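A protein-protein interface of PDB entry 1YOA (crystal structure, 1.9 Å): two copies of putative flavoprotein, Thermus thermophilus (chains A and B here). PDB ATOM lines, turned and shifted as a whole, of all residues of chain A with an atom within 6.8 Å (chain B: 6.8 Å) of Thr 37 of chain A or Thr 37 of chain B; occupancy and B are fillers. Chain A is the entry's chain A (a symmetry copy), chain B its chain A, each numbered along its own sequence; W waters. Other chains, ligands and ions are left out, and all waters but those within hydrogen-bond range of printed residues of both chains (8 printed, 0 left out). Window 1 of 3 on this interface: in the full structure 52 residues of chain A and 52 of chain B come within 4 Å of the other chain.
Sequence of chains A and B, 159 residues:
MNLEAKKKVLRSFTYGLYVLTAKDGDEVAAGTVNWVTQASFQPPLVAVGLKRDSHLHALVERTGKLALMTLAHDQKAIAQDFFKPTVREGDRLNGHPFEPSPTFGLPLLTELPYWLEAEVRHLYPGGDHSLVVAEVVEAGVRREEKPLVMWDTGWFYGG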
ATOM      1  N   LEU A  10     -31.692 -16.707 -23.073  1.00  0.00           N
ATOM      2  CA  LEU A  10     -30.310 -17.008 -22.682  1.00  0.00           C
ATOM      3  C   LEU A  10     -29.377 -16.920 -23.900  1.00  0.00           C
ATOM      4  O   LEU A  10     -28.229 -16.516 -23.766  1.00  0.00           O
ATOM      5  CB  LEU A  10     -30.205 -18.344 -21.942  1.00  0.00           C
ATOM      6  CG  LEU A  10     -30.864 -18.446 -20.554  1.00  0.00           C
ATOM      7  CD1 LEU A  10     -30.849 -19.858 -19.974  1.00  0.00           C
ATOM      8  CD2 LEU A  10     -30.218 -17.478 -19.544  1.00  0.00           C
ATOM      9  N   PHE A  13     -27.613 -13.454 -24.896  1.00  0.00           N
ATOM     10  CA  PHE A  13     -26.458 -12.991 -24.100  1.00  0.00           C
ATOM     11  C   PHE A  13     -25.245 -12.905 -25.020  1.00  0.00           C
ATOM     12  O   PHE A  13     -25.063 -13.757 -25.916  1.00  0.00           O
ATOM     13  CB  PHE A  13     -26.129 -13.953 -22.948  1.00  0.00           C
ATOM     14  CG  PHE A  13     -27.081 -13.911 -21.769  1.00  0.00           C
ATOM     15  CD1 PHE A  13     -28.352 -13.351 -21.854  1.00  0.00           C
ATOM     16  CD2 PHE A  13     -26.685 -14.483 -20.575  1.00  0.00           C
ATOM     17  CE1 PHE A  13     -29.190 -13.357 -20.752  1.00  0.00           C
ATOM     18  CE2 PHE A  13     -27.531 -14.486 -19.473  1.00  0.00           C
ATOM     19  CZ  PHE A  13     -28.785 -13.928 -19.584  1.00  0.00           C
ATOM     20  N   THR A  14     -24.416 -11.901 -24.781  1.00  0.00           N
ATOM     21  CA  THR A  14     -23.222 -11.636 -25.589  1.00  0.00           C
ATOM     22  C   THR A  14     -21.986 -12.132 -24.858  1.00  0.00           C
ATOM     23  O   THR A  14     -21.828 -11.867 -23.667  1.00  0.00           O
ATOM     24  CB  THR A  14     -23.130 -10.139 -25.828  1.00  0.00           C
ATOM     25  OG1 THR A  14     -24.139  -9.754 -26.772  1.00  0.00           O
ATOM     26  CG2 THR A  14     -21.788  -9.740 -26.485  1.00  0.00           C
ATOM     27  N   TYR A  15     -21.134 -12.881 -25.569  1.00  0.00           N
ATOM     28  CA  TYR A  15     -19.883 -13.370 -25.006  1.00  0.00           C
ATOM     29  C   TYR A  15     -18.686 -13.168 -25.921  1.00  0.00           C
ATOM     30  O   TYR A  15     -18.818 -13.022 -27.127  1.00  0.00           O
ATOM     31  CB  TYR A  15     -19.989 -14.876 -24.748  1.00  0.00           C
ATOM     32  CG  TYR A  15     -21.119 -15.310 -23.864  1.00  0.00           C
ATOM     33  CD1 TYR A  15     -22.275 -15.896 -24.403  1.00  0.00           C
ATOM     34  CD2 TYR A  15     -21.034 -15.177 -22.495  1.00  0.00           C
ATOM     35  CE1 TYR A  15     -23.307 -16.343 -23.577  1.00  0.00           C
ATOM     36  CE2 TYR A  15     -22.053 -15.614 -21.669  1.00  0.00           C
ATOM     37  CZ  TYR A  15     -23.178 -16.203 -22.221  1.00  0.00           C
ATOM     38  OH  TYR A  15     -24.160 -16.615 -21.383  1.00  0.00           O
ATOM     39  N   TYR A  18     -12.526 -17.319 -25.445  1.00  0.00           N
ATOM     40  CA  TYR A  18     -11.314 -17.382 -24.623  1.00  0.00           C
ATOM     41  C   TYR A  18     -10.835 -18.826 -24.610  1.00  0.00           C
ATOM     42  O   TYR A  18     -11.628 -19.765 -24.860  1.00  0.00           O
ATOM     43  CB  TYR A  18     -11.580 -16.949 -23.164  1.00  0.00           C
ATOM     44  CG  TYR A  18     -12.393 -15.691 -23.014  1.00  0.00           C
ATOM     45  CD1 TYR A  18     -11.777 -14.447 -22.916  1.00  0.00           C
ATOM     46  CD2 TYR A  18     -13.785 -15.736 -23.028  1.00  0.00           C
ATOM     47  CE1 TYR A  18     -12.553 -13.271 -22.821  1.00  0.00           C
ATOM     48  CE2 TYR A  18     -14.555 -14.567 -22.922  1.00  0.00           C
ATOM     49  CZ  TYR A  18     -13.938 -13.355 -22.815  1.00  0.00           C
ATOM     50  OH  TYR A  18     -14.689 -12.194 -22.702  1.00  0.00           O
ATOM     51  N   ASN A  34     -16.794 -19.587 -23.366  1.00  0.00           N
ATOM     52  CA  ASN A  34     -17.467 -18.309 -23.480  1.00  0.00           C
ATOM     53  C   ASN A  34     -18.024 -17.737 -22.179  1.00  0.00           C
ATOM     54  O   ASN A  34     -18.191 -16.521 -22.083  1.00  0.00           O
ATOM     55  CB  ASN A  34     -18.516 -18.344 -24.570  1.00  0.00           C
ATOM     56  CG  ASN A  34     -19.723 -19.089 -24.208  1.00  0.00           C
ATOM     57  OD1 ASN A  34     -20.833 -18.625 -24.473  1.00  0.00           O
ATOM     58  ND2 ASN A  34     -19.561 -20.287 -23.680  1.00  0.00           N
ATOM     59  N   TRP A  35     -18.364 -18.596 -21.234  1.00  0.00           N
ATOM     60  CA  TRP A  35     -19.041 -18.172 -20.000  1.00  0.00           C
ATOM     61  C   TRP A  35     -18.032 -17.582 -19.025  1.00  0.00           C
ATOM     62  O   TRP A  35     -17.614 -18.206 -18.066  1.00  0.00           O
ATOM     63  CB  TRP A  35     -19.809 -19.353 -19.398  1.00  0.00           C
ATOM     64  CG  TRP A  35     -21.010 -19.765 -20.196  1.00  0.00           C
ATOM     65  CD1 TRP A  35     -21.517 -19.175 -21.286  1.00  0.00           C
ATOM     66  CD2 TRP A  35     -21.875 -20.881 -19.903  1.00  0.00           C
ATOM     67  NE1 TRP A  35     -22.633 -19.849 -21.716  1.00  0.00           N
ATOM     68  CE2 TRP A  35     -22.877 -20.892 -20.864  1.00  0.00           C
ATOM     69  CE3 TRP A  35     -21.885 -21.861 -18.913  1.00  0.00           C
ATOM     70  CZ2 TRP A  35     -23.877 -21.877 -20.904  1.00  0.00           C
ATOM     71  CZ3 TRP A  35     -22.901 -22.844 -18.931  1.00  0.00           C
ATOM     72  CH2 TRP A  35     -23.877 -22.825 -19.903  1.00  0.00           C
ATOM     73  N   VAL A  36     -17.663 -16.330 -19.286  1.00  0.00           N
ATOM     74  CA  VAL A  36     -16.581 -15.665 -18.563  1.00  0.00           C
ATOM     75  C   VAL A  36     -17.029 -14.216 -18.285  1.00  0.00           C
ATOM     76  O   VAL A  36     -17.505 -13.505 -19.203  1.00  0.00           O
ATOM     77  CB  VAL A  36     -15.286 -15.619 -19.421  1.00  0.00           C
ATOM     78  CG1 VAL A  36     -14.206 -14.764 -18.781  1.00  0.00           C
ATOM     79  CG2 VAL A  36     -14.756 -17.017 -19.708  1.00  0.00           C
ATOM     80  N   THR A  37     -16.836 -13.772 -17.052  1.00  0.00           N
ATOM     81  CA  THR A  37     -17.065 -12.362 -16.729  1.00  0.00           C
ATOM     82  C   THR A  37     -16.126 -11.918 -15.594  1.00  0.00           C
ATOM     83  O   THR A  37     -15.793 -12.693 -14.728  1.00  0.00           O
ATOM     84  CB  THR A  37     -18.544 -12.084 -16.358  1.00  0.00           C
ATOM     85  OG1 THR A  37     -18.715 -10.698 -15.950  1.00  0.00           O
ATOM     86  CG2 THR A  37     -18.977 -12.908 -15.138  1.00  0.00           C
ATOM     87  N   GLN A  38     -15.745 -10.645 -15.582  1.00  0.00           N
ATOM     88  CA  GLN A  38     -15.108 -10.092 -14.394  1.00  0.00           C
ATOM     89  C   GLN A  38     -16.172 -10.103 -13.252  1.00  0.00           C
ATOM     90  O   GLN A  38     -17.390 -10.062 -13.514  1.00  0.00           O
ATOM     91  CB  GLN A  38     -14.522  -8.706 -14.719  1.00  0.00           C
ATOM     92  CG  GLN A  38     -13.779  -8.075 -13.570  1.00  0.00           C
ATOM     93  CD  GLN A  38     -12.925  -6.886 -13.908  1.00  0.00           C
ATOM     94  OE1 GLN A  38     -12.339  -6.274 -12.961  1.00  0.00           O
ATOM     95  NE2 GLN A  38     -12.886  -6.486 -15.150  1.00  0.00           N
ATOM     96  N   ALA A  39     -15.726 -10.221 -11.998  1.00  0.00           N
ATOM     97  CA  ALA A  39     -16.609 -10.334 -10.842  1.00  0.00           C
ATOM     98  C   ALA A  39     -16.229  -9.419  -9.634  1.00  0.00           C
ATOM     99  O   ALA A  39     -16.788  -9.577  -8.577  1.00  0.00           O
ATOM    100  CB  ALA A  39     -16.696 -11.764 -10.406  1.00  0.00           C
ATOM    101  N   SER A  40     -15.280  -8.521  -9.835  1.00  0.00           N
ATOM    102  CA  SER A  40     -14.910  -7.444  -8.868  1.00  0.00           C
ATOM    103  C   SER A  40     -13.652  -6.726  -9.439  1.00  0.00           C
ATOM    104  O   SER A  40     -12.909  -7.296 -10.219  1.00  0.00           O
ATOM    105  CB  SER A  40     -14.821  -8.009  -7.422  1.00  0.00           C
ATOM    106  OG  SER A  40     -13.778  -7.422  -6.676  1.00  0.00           O
ATOM    107  N   LEU A  45     -11.237 -10.191  -9.727  1.00  0.00           N
ATOM    108  CA  LEU A  45     -11.812 -11.521  -9.845  1.00  0.00           C
ATOM    109  C   LEU A  45     -12.384 -11.790 -11.224  1.00  0.00           C
ATOM    110  O   LEU A  45     -12.963 -10.914 -11.837  1.00  0.00           O
ATOM    111  CB  LEU A  45     -12.922 -11.690  -8.814  1.00  0.00           C
ATOM    112  CG  LEU A  45     -12.507 -11.539  -7.343  1.00  0.00           C
ATOM    113  CD1 LEU A  45     -13.717 -11.649  -6.508  1.00  0.00           C
ATOM    114  CD2 LEU A  45     -11.466 -12.573  -6.926  1.00  0.00           C
ATOM    115  N   VAL A  46     -12.205 -13.012 -11.714  1.00  0.00           N
ATOM    116  CA  VAL A  46     -12.835 -13.464 -12.949  1.00  0.00           C
ATOM    117  C   VAL A  46     -13.685 -14.654 -12.544  1.00  0.00           C
ATOM    118  O   VAL A  46     -13.281 -15.449 -11.707  1.00  0.00           O
ATOM    119  CB  VAL A  46     -11.819 -13.892 -14.010  1.00  0.00           C
ATOM    120  CG1 VAL A  46     -10.893 -14.943 -13.484  1.00  0.00           C
ATOM    121  CG2 VAL A  46     -12.506 -14.442 -15.271  1.00  0.00           C
ATOM    122  N   ALA A  47     -14.869 -14.745 -13.117  1.00  0.00           N
ATOM    123  CA  ALA A  47     -15.752 -15.896 -12.933  1.00  0.00           C
ATOM    124  C   ALA A  47     -15.875 -16.649 -14.253  1.00  0.00           C
ATOM    125  O   ALA A  47     -16.035 -16.040 -15.313  1.00  0.00           O
ATOM    126  CB  ALA A  47     -17.106 -15.452 -12.483  1.00  0.00           C
ATOM    127  N   VAL A  48     -15.817 -17.980 -14.181  1.00  0.00           N
ATOM    128  CA  VAL A  48     -15.926 -18.853 -15.358  1.00  0.00           C
ATOM    129  C   VAL A  48     -16.927 -19.979 -15.082  1.00  0.00           C
ATOM    130  O   VAL A  48     -16.837 -20.645 -14.052  1.00  0.00           O
ATOM    131  CB  VAL A  48     -14.585 -19.490 -15.720  1.00  0.00           C
ATOM    132  CG1 VAL A  48     -14.691 -20.261 -17.031  1.00  0.00           C
ATOM    133  CG2 VAL A  48     -13.502 -18.423 -15.838  1.00  0.00           C
ATOM    134  N   GLY A  49     -17.873 -20.175 -15.997  1.00  0.00           N
ATOM    135  CA  GLY A  49     -18.759 -21.337 -15.984  1.00  0.00           C
ATOM    136  C   GLY A  49     -18.066 -22.517 -16.666  1.00  0.00           C
ATOM    137  O   GLY A  49     -17.890 -22.508 -17.894  1.00  0.00           O
ATOM    138  N   LEU A 131     -19.450 -22.635 -11.214  1.00  0.00           N
ATOM    139  CA  LEU A 131     -19.022 -21.254 -11.353  1.00  0.00           C
ATOM    140  C   LEU A 131     -17.756 -21.080 -10.507  1.00  0.00           C
ATOM    141  O   LEU A 131     -17.779 -21.133  -9.278  1.00  0.00           O
ATOM    142  CB  LEU A 131     -20.164 -20.313 -10.977  1.00  0.00           C
ATOM    143  CG  LEU A 131     -20.044 -18.844 -11.414  1.00  0.00           C
ATOM    144  CD1 LEU A 131     -19.927 -18.665 -12.913  1.00  0.00           C
ATOM    145  CD2 LEU A 131     -21.251 -18.115 -10.912  1.00  0.00           C
ATOM    146  N   LEU B  10      -8.266  -7.483 -18.667  1.00  0.00           N
ATOM    147  CA  LEU B  10      -9.663  -7.546 -18.220  1.00  0.00           C
ATOM    148  C   LEU B  10     -10.559  -6.705 -19.143  1.00  0.00           C
ATOM    149  O   LEU B  10     -11.705  -7.064 -19.380  1.00  0.00           O
ATOM    150  CB  LEU B  10      -9.805  -7.174 -16.743  1.00  0.00           C
ATOM    151  CG  LEU B  10      -9.188  -8.126 -15.702  1.00  0.00           C
ATOM    152  CD1 LEU B  10      -9.237  -7.585 -14.276  1.00  0.00           C
ATOM    153  CD2 LEU B  10      -9.850  -9.516 -15.739  1.00  0.00           C
ATOM    154  N   PHE B  13     -12.250  -8.321 -22.405  1.00  0.00           N
ATOM    155  CA  PHE B  13     -13.421  -9.204 -22.234  1.00  0.00           C
ATOM    156  C   PHE B  13     -14.606  -8.576 -22.959  1.00  0.00           C
ATOM    157  O   PHE B  13     -14.773  -7.338 -22.953  1.00  0.00           O
ATOM    158  CB  PHE B  13     -13.795  -9.386 -20.754  1.00  0.00           C
ATOM    159  CG  PHE B  13     -12.878 -10.287 -19.953  1.00  0.00           C
ATOM    160  CD1 PHE B  13     -11.597 -10.623 -20.383  1.00  0.00           C
ATOM    161  CD2 PHE B  13     -13.314 -10.764 -18.732  1.00  0.00           C
ATOM    162  CE1 PHE B  13     -10.791 -11.435 -19.603  1.00  0.00           C
ATOM    163  CE2 PHE B  13     -12.501 -11.578 -17.953  1.00  0.00           C
ATOM    164  CZ  PHE B  13     -11.237 -11.893 -18.400  1.00  0.00           C
ATOM    165  N   THR B  14     -15.429  -9.426 -23.553  1.00  0.00           N
ATOM    166  CA  THR B  14     -16.596  -9.002 -24.332  1.00  0.00           C
ATOM    167  C   THR B  14     -17.859  -9.182 -23.507  1.00  0.00           C
ATOM    168  O   THR B  14     -18.048 -10.231 -22.892  1.00  0.00           O
ATOM    169  CB  THR B  14     -16.663  -9.848 -25.591  1.00  0.00           C
ATOM    170  OG1 THR B  14     -15.622  -9.434 -26.487  1.00  0.00           O
ATOM    171  CG2 THR B  14     -17.981  -9.624 -26.369  1.00  0.00           C
ATOM    172  N   TYR B  15     -18.699  -8.140 -23.469  1.00  0.00           N
ATOM    173  CA  TYR B  15     -19.972  -8.202 -22.763  1.00  0.00           C
ATOM    174  C   TYR B  15     -21.140  -7.657 -23.570  1.00  0.00           C
ATOM    175  O   TYR B  15     -20.971  -6.878 -24.495  1.00  0.00           O
ATOM    176  CB  TYR B  15     -19.892  -7.364 -21.485  1.00  0.00           C
ATOM    177  CG  TYR B  15     -18.793  -7.728 -20.531  1.00  0.00           C
ATOM    178  CD1 TYR B  15     -17.630  -6.948 -20.438  1.00  0.00           C
ATOM    179  CD2 TYR B  15     -18.916  -8.817 -19.697  1.00  0.00           C
ATOM    180  CE1 TYR B  15     -16.628  -7.258 -19.518  1.00  0.00           C
ATOM    181  CE2 TYR B  15     -17.927  -9.135 -18.785  1.00  0.00           C
ATOM    182  CZ  TYR B  15     -16.794  -8.343 -18.699  1.00  0.00           C
ATOM    183  OH  TYR B  15     -15.841  -8.687 -17.798  1.00  0.00           O
ATOM    184  N   TYR B  18     -27.362  -5.093 -20.389  1.00  0.00           N
ATOM    185  CA  TYR B  18     -28.598  -5.636 -19.817  1.00  0.00           C
ATOM    186  C   TYR B  18     -29.095  -4.653 -18.768  1.00  0.00           C
ATOM    187  O   TYR B  18     -28.307  -3.840 -18.229  1.00  0.00           O
ATOM    188  CB  TYR B  18     -28.368  -7.000 -19.131  1.00  0.00           C
ATOM    189  CG  TYR B  18     -27.545  -7.979 -19.923  1.00  0.00           C
ATOM    190  CD1 TYR B  18     -28.147  -8.892 -20.784  1.00  0.00           C
ATOM    191  CD2 TYR B  18     -26.154  -7.955 -19.861  1.00  0.00           C
ATOM    192  CE1 TYR B  18     -27.360  -9.774 -21.555  1.00  0.00           C
ATOM    193  CE2 TYR B  18     -25.372  -8.841 -20.620  1.00  0.00           C
ATOM    194  CZ  TYR B  18     -25.977  -9.739 -21.450  1.00  0.00           C
ATOM    195  OH  TYR B  18     -25.215 -10.623 -22.200  1.00  0.00           O
ATOM    196  N   ASN B  34     -23.184  -5.117 -17.191  1.00  0.00           N
ATOM    197  CA  ASN B  34     -22.493  -5.915 -18.184  1.00  0.00           C
ATOM    198  C   ASN B  34     -21.966  -7.263 -17.698  1.00  0.00           C
ATOM    199  O   ASN B  34     -21.786  -8.165 -18.516  1.00  0.00           O
ATOM    200  CB  ASN B  34     -21.412  -5.107 -18.872  1.00  0.00           C
ATOM    201  CG  ASN B  34     -20.226  -4.879 -18.046  1.00  0.00           C
ATOM    202  OD1 ASN B  34     -19.103  -5.015 -18.534  1.00  0.00           O
ATOM    203  ND2 ASN B  34     -20.419  -4.445 -16.815  1.00  0.00           N
ATOM    204  N   TRP B  35     -21.664  -7.370 -16.416  1.00  0.00           N
ATOM    205  CA  TRP B  35     -21.017  -8.570 -15.864  1.00  0.00           C
ATOM    206  C   TRP B  35     -22.046  -9.672 -15.659  1.00  0.00           C
ATOM    207  O   TRP B  35     -22.500  -9.942 -14.560  1.00  0.00           O
ATOM    208  CB  TRP B  35     -20.281  -8.213 -14.568  1.00  0.00           C
ATOM    209  CG  TRP B  35     -19.064  -7.363 -14.777  1.00  0.00           C
ATOM    210  CD1 TRP B  35     -18.518  -6.976 -15.938  1.00  0.00           C
ATOM    211  CD2 TRP B  35     -18.221  -6.827 -13.738  1.00  0.00           C
ATOM    212  NE1 TRP B  35     -17.399  -6.217 -15.707  1.00  0.00           N
ATOM    213  CE2 TRP B  35     -17.192  -6.130 -14.357  1.00  0.00           C
ATOM    214  CE3 TRP B  35     -18.252  -6.881 -12.346  1.00  0.00           C
ATOM    215  CZ2 TRP B  35     -16.203  -5.441 -13.635  1.00  0.00           C
ATOM    216  CZ3 TRP B  35     -17.248  -6.209 -11.611  1.00  0.00           C
ATOM    217  CH2 TRP B  35     -16.244  -5.524 -12.260  1.00  0.00           C
ATOM    218  N   VAL B  36     -22.392 -10.332 -16.762  1.00  0.00           N
ATOM    219  CA  VAL B  36     -23.486 -11.301 -16.786  1.00  0.00           C
ATOM    220  C   VAL B  36     -23.028 -12.499 -17.642  1.00  0.00           C
ATOM    221  O   VAL B  36     -22.517 -12.319 -18.773  1.00  0.00           O
ATOM    222  CB  VAL B  36     -24.755 -10.689 -17.442  1.00  0.00           C
ATOM    223  CG1 VAL B  36     -25.842 -11.727 -17.661  1.00  0.00           C
ATOM    224  CG2 VAL B  36     -25.294  -9.518 -16.632  1.00  0.00           C
ATOM    225  N   THR B  37     -23.251 -13.700 -17.130  1.00  0.00           N
ATOM    226  CA  THR B  37     -23.014 -14.902 -17.933  1.00  0.00           C
ATOM    227  C   THR B  37     -23.979 -16.023 -17.511  1.00  0.00           C
ATOM    228  O   THR B  37     -24.347 -16.122 -16.363  1.00  0.00           O
ATOM    229  CB  THR B  37     -21.543 -15.381 -17.841  1.00  0.00           C
ATOM    230  OG1 THR B  37     -21.366 -16.628 -18.570  1.00  0.00           O
ATOM    231  CG2 THR B  37     -21.155 -15.714 -16.394  1.00  0.00           C
ATOM    232  N   GLN B  38     -24.345 -16.895 -18.443  1.00  0.00           N
ATOM    233  CA  GLN B  38     -25.009 -18.133 -18.054  1.00  0.00           C
ATOM    234  C   GLN B  38     -23.977 -18.973 -17.237  1.00  0.00           C
ATOM    235  O   GLN B  38     -22.752 -18.825 -17.410  1.00  0.00           O
ATOM    236  CB  GLN B  38     -25.568 -18.835 -19.305  1.00  0.00           C
ATOM    237  CG  GLN B  38     -26.335 -20.095 -19.004  1.00  0.00           C
ATOM    238  CD  GLN B  38     -27.165 -20.650 -20.128  1.00  0.00           C
ATOM    239  OE1 GLN B  38     -27.769 -21.752 -19.946  1.00  0.00           O
ATOM    240  NE2 GLN B  38     -27.162 -20.016 -21.269  1.00  0.00           N
ATOM    241  N   ALA B  39     -24.461 -19.803 -16.308  1.00  0.00           N
ATOM    242  CA  ALA B  39     -23.613 -20.582 -15.412  1.00  0.00           C
ATOM    243  C   ALA B  39     -24.016 -22.084 -15.267  1.00  0.00           C
ATOM    244  O   ALA B  39     -23.489 -22.755 -14.414  1.00  0.00           O
ATOM    245  CB  ALA B  39     -23.557 -19.924 -14.067  1.00  0.00           C
ATOM    246  N   SER B  40     -24.948 -22.539 -16.087  1.00  0.00           N
ATOM    247  CA  SER B  40     -25.332 -23.975 -16.225  1.00  0.00           C
ATOM    248  C   SER B  40     -26.564 -24.033 -17.174  1.00  0.00           C
ATOM    249  O   SER B  40     -27.292 -23.065 -17.311  1.00  0.00           O
ATOM    250  CB  SER B  40     -25.470 -24.645 -14.828  1.00  0.00           C
ATOM    251  OG  SER B  40     -26.526 -25.577 -14.777  1.00  0.00           O
ATOM    252  N   LEU B  45     -29.013 -21.427 -14.909  1.00  0.00           N
ATOM    253  CA  LEU B  45     -28.451 -20.439 -14.002  1.00  0.00           C
ATOM    254  C   LEU B  45     -27.844 -19.255 -14.730  1.00  0.00           C
ATOM    255  O   LEU B  45     -27.236 -19.413 -15.771  1.00  0.00           O
ATOM    256  CB  LEU B  45     -27.373 -21.091 -13.143  1.00  0.00           C
ATOM    257  CG  LEU B  45     -27.828 -22.264 -12.261  1.00  0.00           C
ATOM    258  CD1 LEU B  45     -26.644 -22.813 -11.577  1.00  0.00           C
ATOM    259  CD2 LEU B  45     -28.894 -21.849 -11.251  1.00  0.00           C
ATOM    260  N   VAL B  46     -28.023 -18.061 -14.176  1.00  0.00           N
ATOM    261  CA  VAL B  46     -27.364 -16.858 -14.671  1.00  0.00           C
ATOM    262  C   VAL B  46     -26.541 -16.352 -13.501  1.00  0.00           C
ATOM    263  O   VAL B  46     -26.979 -16.416 -12.360  1.00  0.00           O
ATOM    264  CB  VAL B  46     -28.355 -15.778 -15.111  1.00  0.00           C
ATOM    265  CG1 VAL B  46     -29.308 -15.433 -14.011  1.00  0.00           C
ATOM    266  CG2 VAL B  46     -27.639 -14.490 -15.550  1.00  0.00           C
ATOM    267  N   ALA B  47     -25.342 -15.886 -13.791  1.00  0.00           N
ATOM    268  CA  ALA B  47     -24.479 -15.246 -12.799  1.00  0.00           C
ATOM    269  C   ALA B  47     -24.328 -13.768 -13.147  1.00  0.00           C
ATOM    270  O   ALA B  47     -24.130 -13.412 -14.310  1.00  0.00           O
ATOM    271  CB  ALA B  47     -23.133 -15.894 -12.777  1.00  0.00           C
ATOM    272  N   VAL B  48     -24.404 -12.912 -12.127  1.00  0.00           N
ATOM    273  CA  VAL B  48     -24.273 -11.457 -12.289  1.00  0.00           C
ATOM    274  C   VAL B  48     -23.293 -10.903 -11.249  1.00  0.00           C
ATOM    275  O   VAL B  48     -23.422 -11.199 -10.063  1.00  0.00           O
ATOM    276  CB  VAL B  48     -25.611 -10.741 -12.109  1.00  0.00           C
ATOM    277  CG1 VAL B  48     -25.476  -9.258 -12.437  1.00  0.00           C
ATOM    278  CG2 VAL B  48     -26.676 -11.370 -13.000  1.00  0.00           C
ATOM    279  N   GLY B  49     -22.324 -10.112 -11.703  1.00  0.00           N
ATOM    280  CA  GLY B  49     -21.453  -9.339 -10.820  1.00  0.00           C
ATOM    281  C   GLY B  49     -22.142  -8.026 -10.443  1.00  0.00           C
ATOM    282  O   GLY B  49     -22.282  -7.133 -11.292  1.00  0.00           O
ATOM    283  N   LEU B 131     -20.917 -11.946  -6.597  1.00  0.00           N
ATOM    284  CA  LEU B 131     -21.322 -12.782  -7.713  1.00  0.00           C
ATOM    285  C   LEU B 131     -22.611 -13.503  -7.300  1.00  0.00           C
ATOM    286  O   LEU B 131     -22.623 -14.365  -6.422  1.00  0.00           O
ATOM    287  CB  LEU B 131     -20.181 -13.713  -8.111  1.00  0.00           C
ATOM    288  CG  LEU B 131     -20.269 -14.396  -9.487  1.00  0.00           C
ATOM    289  CD1 LEU B 131     -20.342 -13.422 -10.643  1.00  0.00           C
ATOM    290  CD2 LEU B 131     -19.069 -15.275  -9.641  1.00  0.00           C
HETATM  291  O   HOH W   1     -22.868 -23.139 -11.398  1.00  0.00           O
HETATM  292  O   HOH W   2     -13.518 -10.838 -25.489  1.00  0.00           O
HETATM  293  O   HOH W   3     -22.529 -10.536 -21.161  1.00  0.00           O
HETATM  294  O   HOH W   4     -26.184 -17.808 -22.614  1.00  0.00           O
HETATM  295  O   HOH W   5     -17.501 -11.510  -6.256  1.00  0.00           O
HETATM  296  O   HOH W   6     -17.402 -12.979 -22.134  1.00  0.00           O
HETATM  297  O   HOH W   7     -26.288  -9.499 -25.125  1.00  0.00           O
HETATM  298  O   HOH W   8     -13.798  -6.998 -17.708  1.00  0.00           O
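N of Gln 38 of chain B sits at hydrogen-bond distance from OH of Tyr 15 of chain A (3.0 Å).
The side-chain hydroxyl of Tyr 18 of chain A is in hydrogen-bond range of the backbone NH of Thr 14 of chain B (3.0 Å).
The backbone NH of Gln 38 of chain A sits at hydrogen-bond distance from the side-chain hydroxyl of Tyr 15 of chain B, at 3.0 Å.
OH of Tyr 18 of chain B lies within hydrogen-bond range of N of Thr 14 of chain A (3.0 Å).
Phe 13 of chain A touches Val 36 of chain B, and with the chains exchanged Val 36 of chain A touches Phe 13 of chain B.
Thr 14 of chain A touches Tyr 15 of chain B, and with the chains exchanged Tyr 15 of chain A touches Thr 14 of chain B.
Leu 131 of chain B touches its own counterpart, Leu 131 of chain A.
Positions printed for both chains: 10, 13, 14, 15, 18, 34, 35, 36, 37, 38, 39, 40, 45, 46, 47, 48, 49 and 131.
Water W8 lies within hydrogen-bond range of the side-chain hydroxyl of Tyr 15 of chain B (2.7 Å), the backbone carbonyl oxygen of Leu 10 of chain B (2.7 Å) and the side-chain amide nitrogen of Gln 38 of chain A (2.8 Å).
Water W7 bridges the side-chain hydroxyl of Thr 14 of chain A (2.7 Å) and the side-chain hydroxyl of Tyr 18 of chain B (3.3 Å).
Printed residues of chain B that touch a printed residue of chain A: Leu 10, Phe 13, Thr 14, Tyr 15, Tyr 18, Trp 35, Val 36, Thr 37, Gln 38, Ala 39, Ser 40, Val 46, Ala 47 and Leu 131.
Hydrophobic or aromatic side chains of chain B that line the printed part of chain A: Leu 10, Phe 13, Tyr 15, Tyr 18, Trp 35, Val 36, Val 46, Ala 47 and Leu 131.
Hydrophobic or aromatic side chains of chain A within 4 Å of the printed part of chain B: Leu 10, Phe 13, Tyr 15, Tyr 18, Trp 35, Val 36, Val 46, Ala 47 and Leu 131.
Along chain A the printed residues that touch a printed residue of chain B span positions 10 to 131.
Among the printed residues, no Asp or Glu carboxylate lies within 4 Å of a Lys or Arg side-chain nitrogen of the other chain.
CB of Leu 10 of chain A touches NE2 of Gln 38 of chain B (3.5 Å).
Phe 13 of chain A touches Gln 38 of chain B.
CE2 of Phe 13 of chain A touches CG2 of Val 46 of chain B, at 3.9 Å.
CG2 of Thr 14 of chain B touches O of Tyr 15 of chain A (3.6 Å).
N of Ser 40 of chain B touches CZ3 of Trp 35 of chain A, 3.5 Å away.
N of Val 36 of chain A touches OG1 of Thr 37 of chain B, at 3.8 Å.
Thr 37 of chain A touches Trp 35 of chain B.
Val 36 of chain B touches Thr 37 of chain A.
The backbone carbonyl oxygen (O) of Trp 35 of chain B is in hydrogen-bond range of the backbone NH (N) of Gly 49 of chain B (2.9 Å).
The backbone NH (N) of Ala 39 of chain A sits at hydrogen-bond distance from the backbone carbonyl oxygen (O) of Leu 45 of chain A, 2.9 Å away.
O of Thr 37 of chain A is in hydrogen-bond range of N of Ala 47 of chain A (2.8 Å).
Of chain B, only Tyr 15 (3.3 Å), Trp 35 (3.1 Å), Val 36 (3.8 Å) and Thr 37 (3.8 Å) come within 4 Å of Thr 37 of chain A.
Of chain A, only Tyr 15 (3.3 Å), Trp 35 (3.1 Å), Val 36 (3.8 Å) and Thr 37 (3.8 Å) come within 4 Å of Thr 37 of chain B.
Of the printed residues of chain B, Tyr 15 of chain A touches Thr 14 (3.6 Å), Thr 37 (3.3 Å) and Gln 38 (3.0 Å).
Of the printed residues of chain A, Val 46 of chain B touches Phe 13.
Of the printed residues of chain A, Trp 35 of chain B touches Thr 37, Gln 38, Ala 39 and Ser 40.
Printed residues of chain B within 4 Å of Val 36 of chain A: Phe 13 and Thr 37.
Asn 34 of chain B touches none of the printed residues of chain A.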
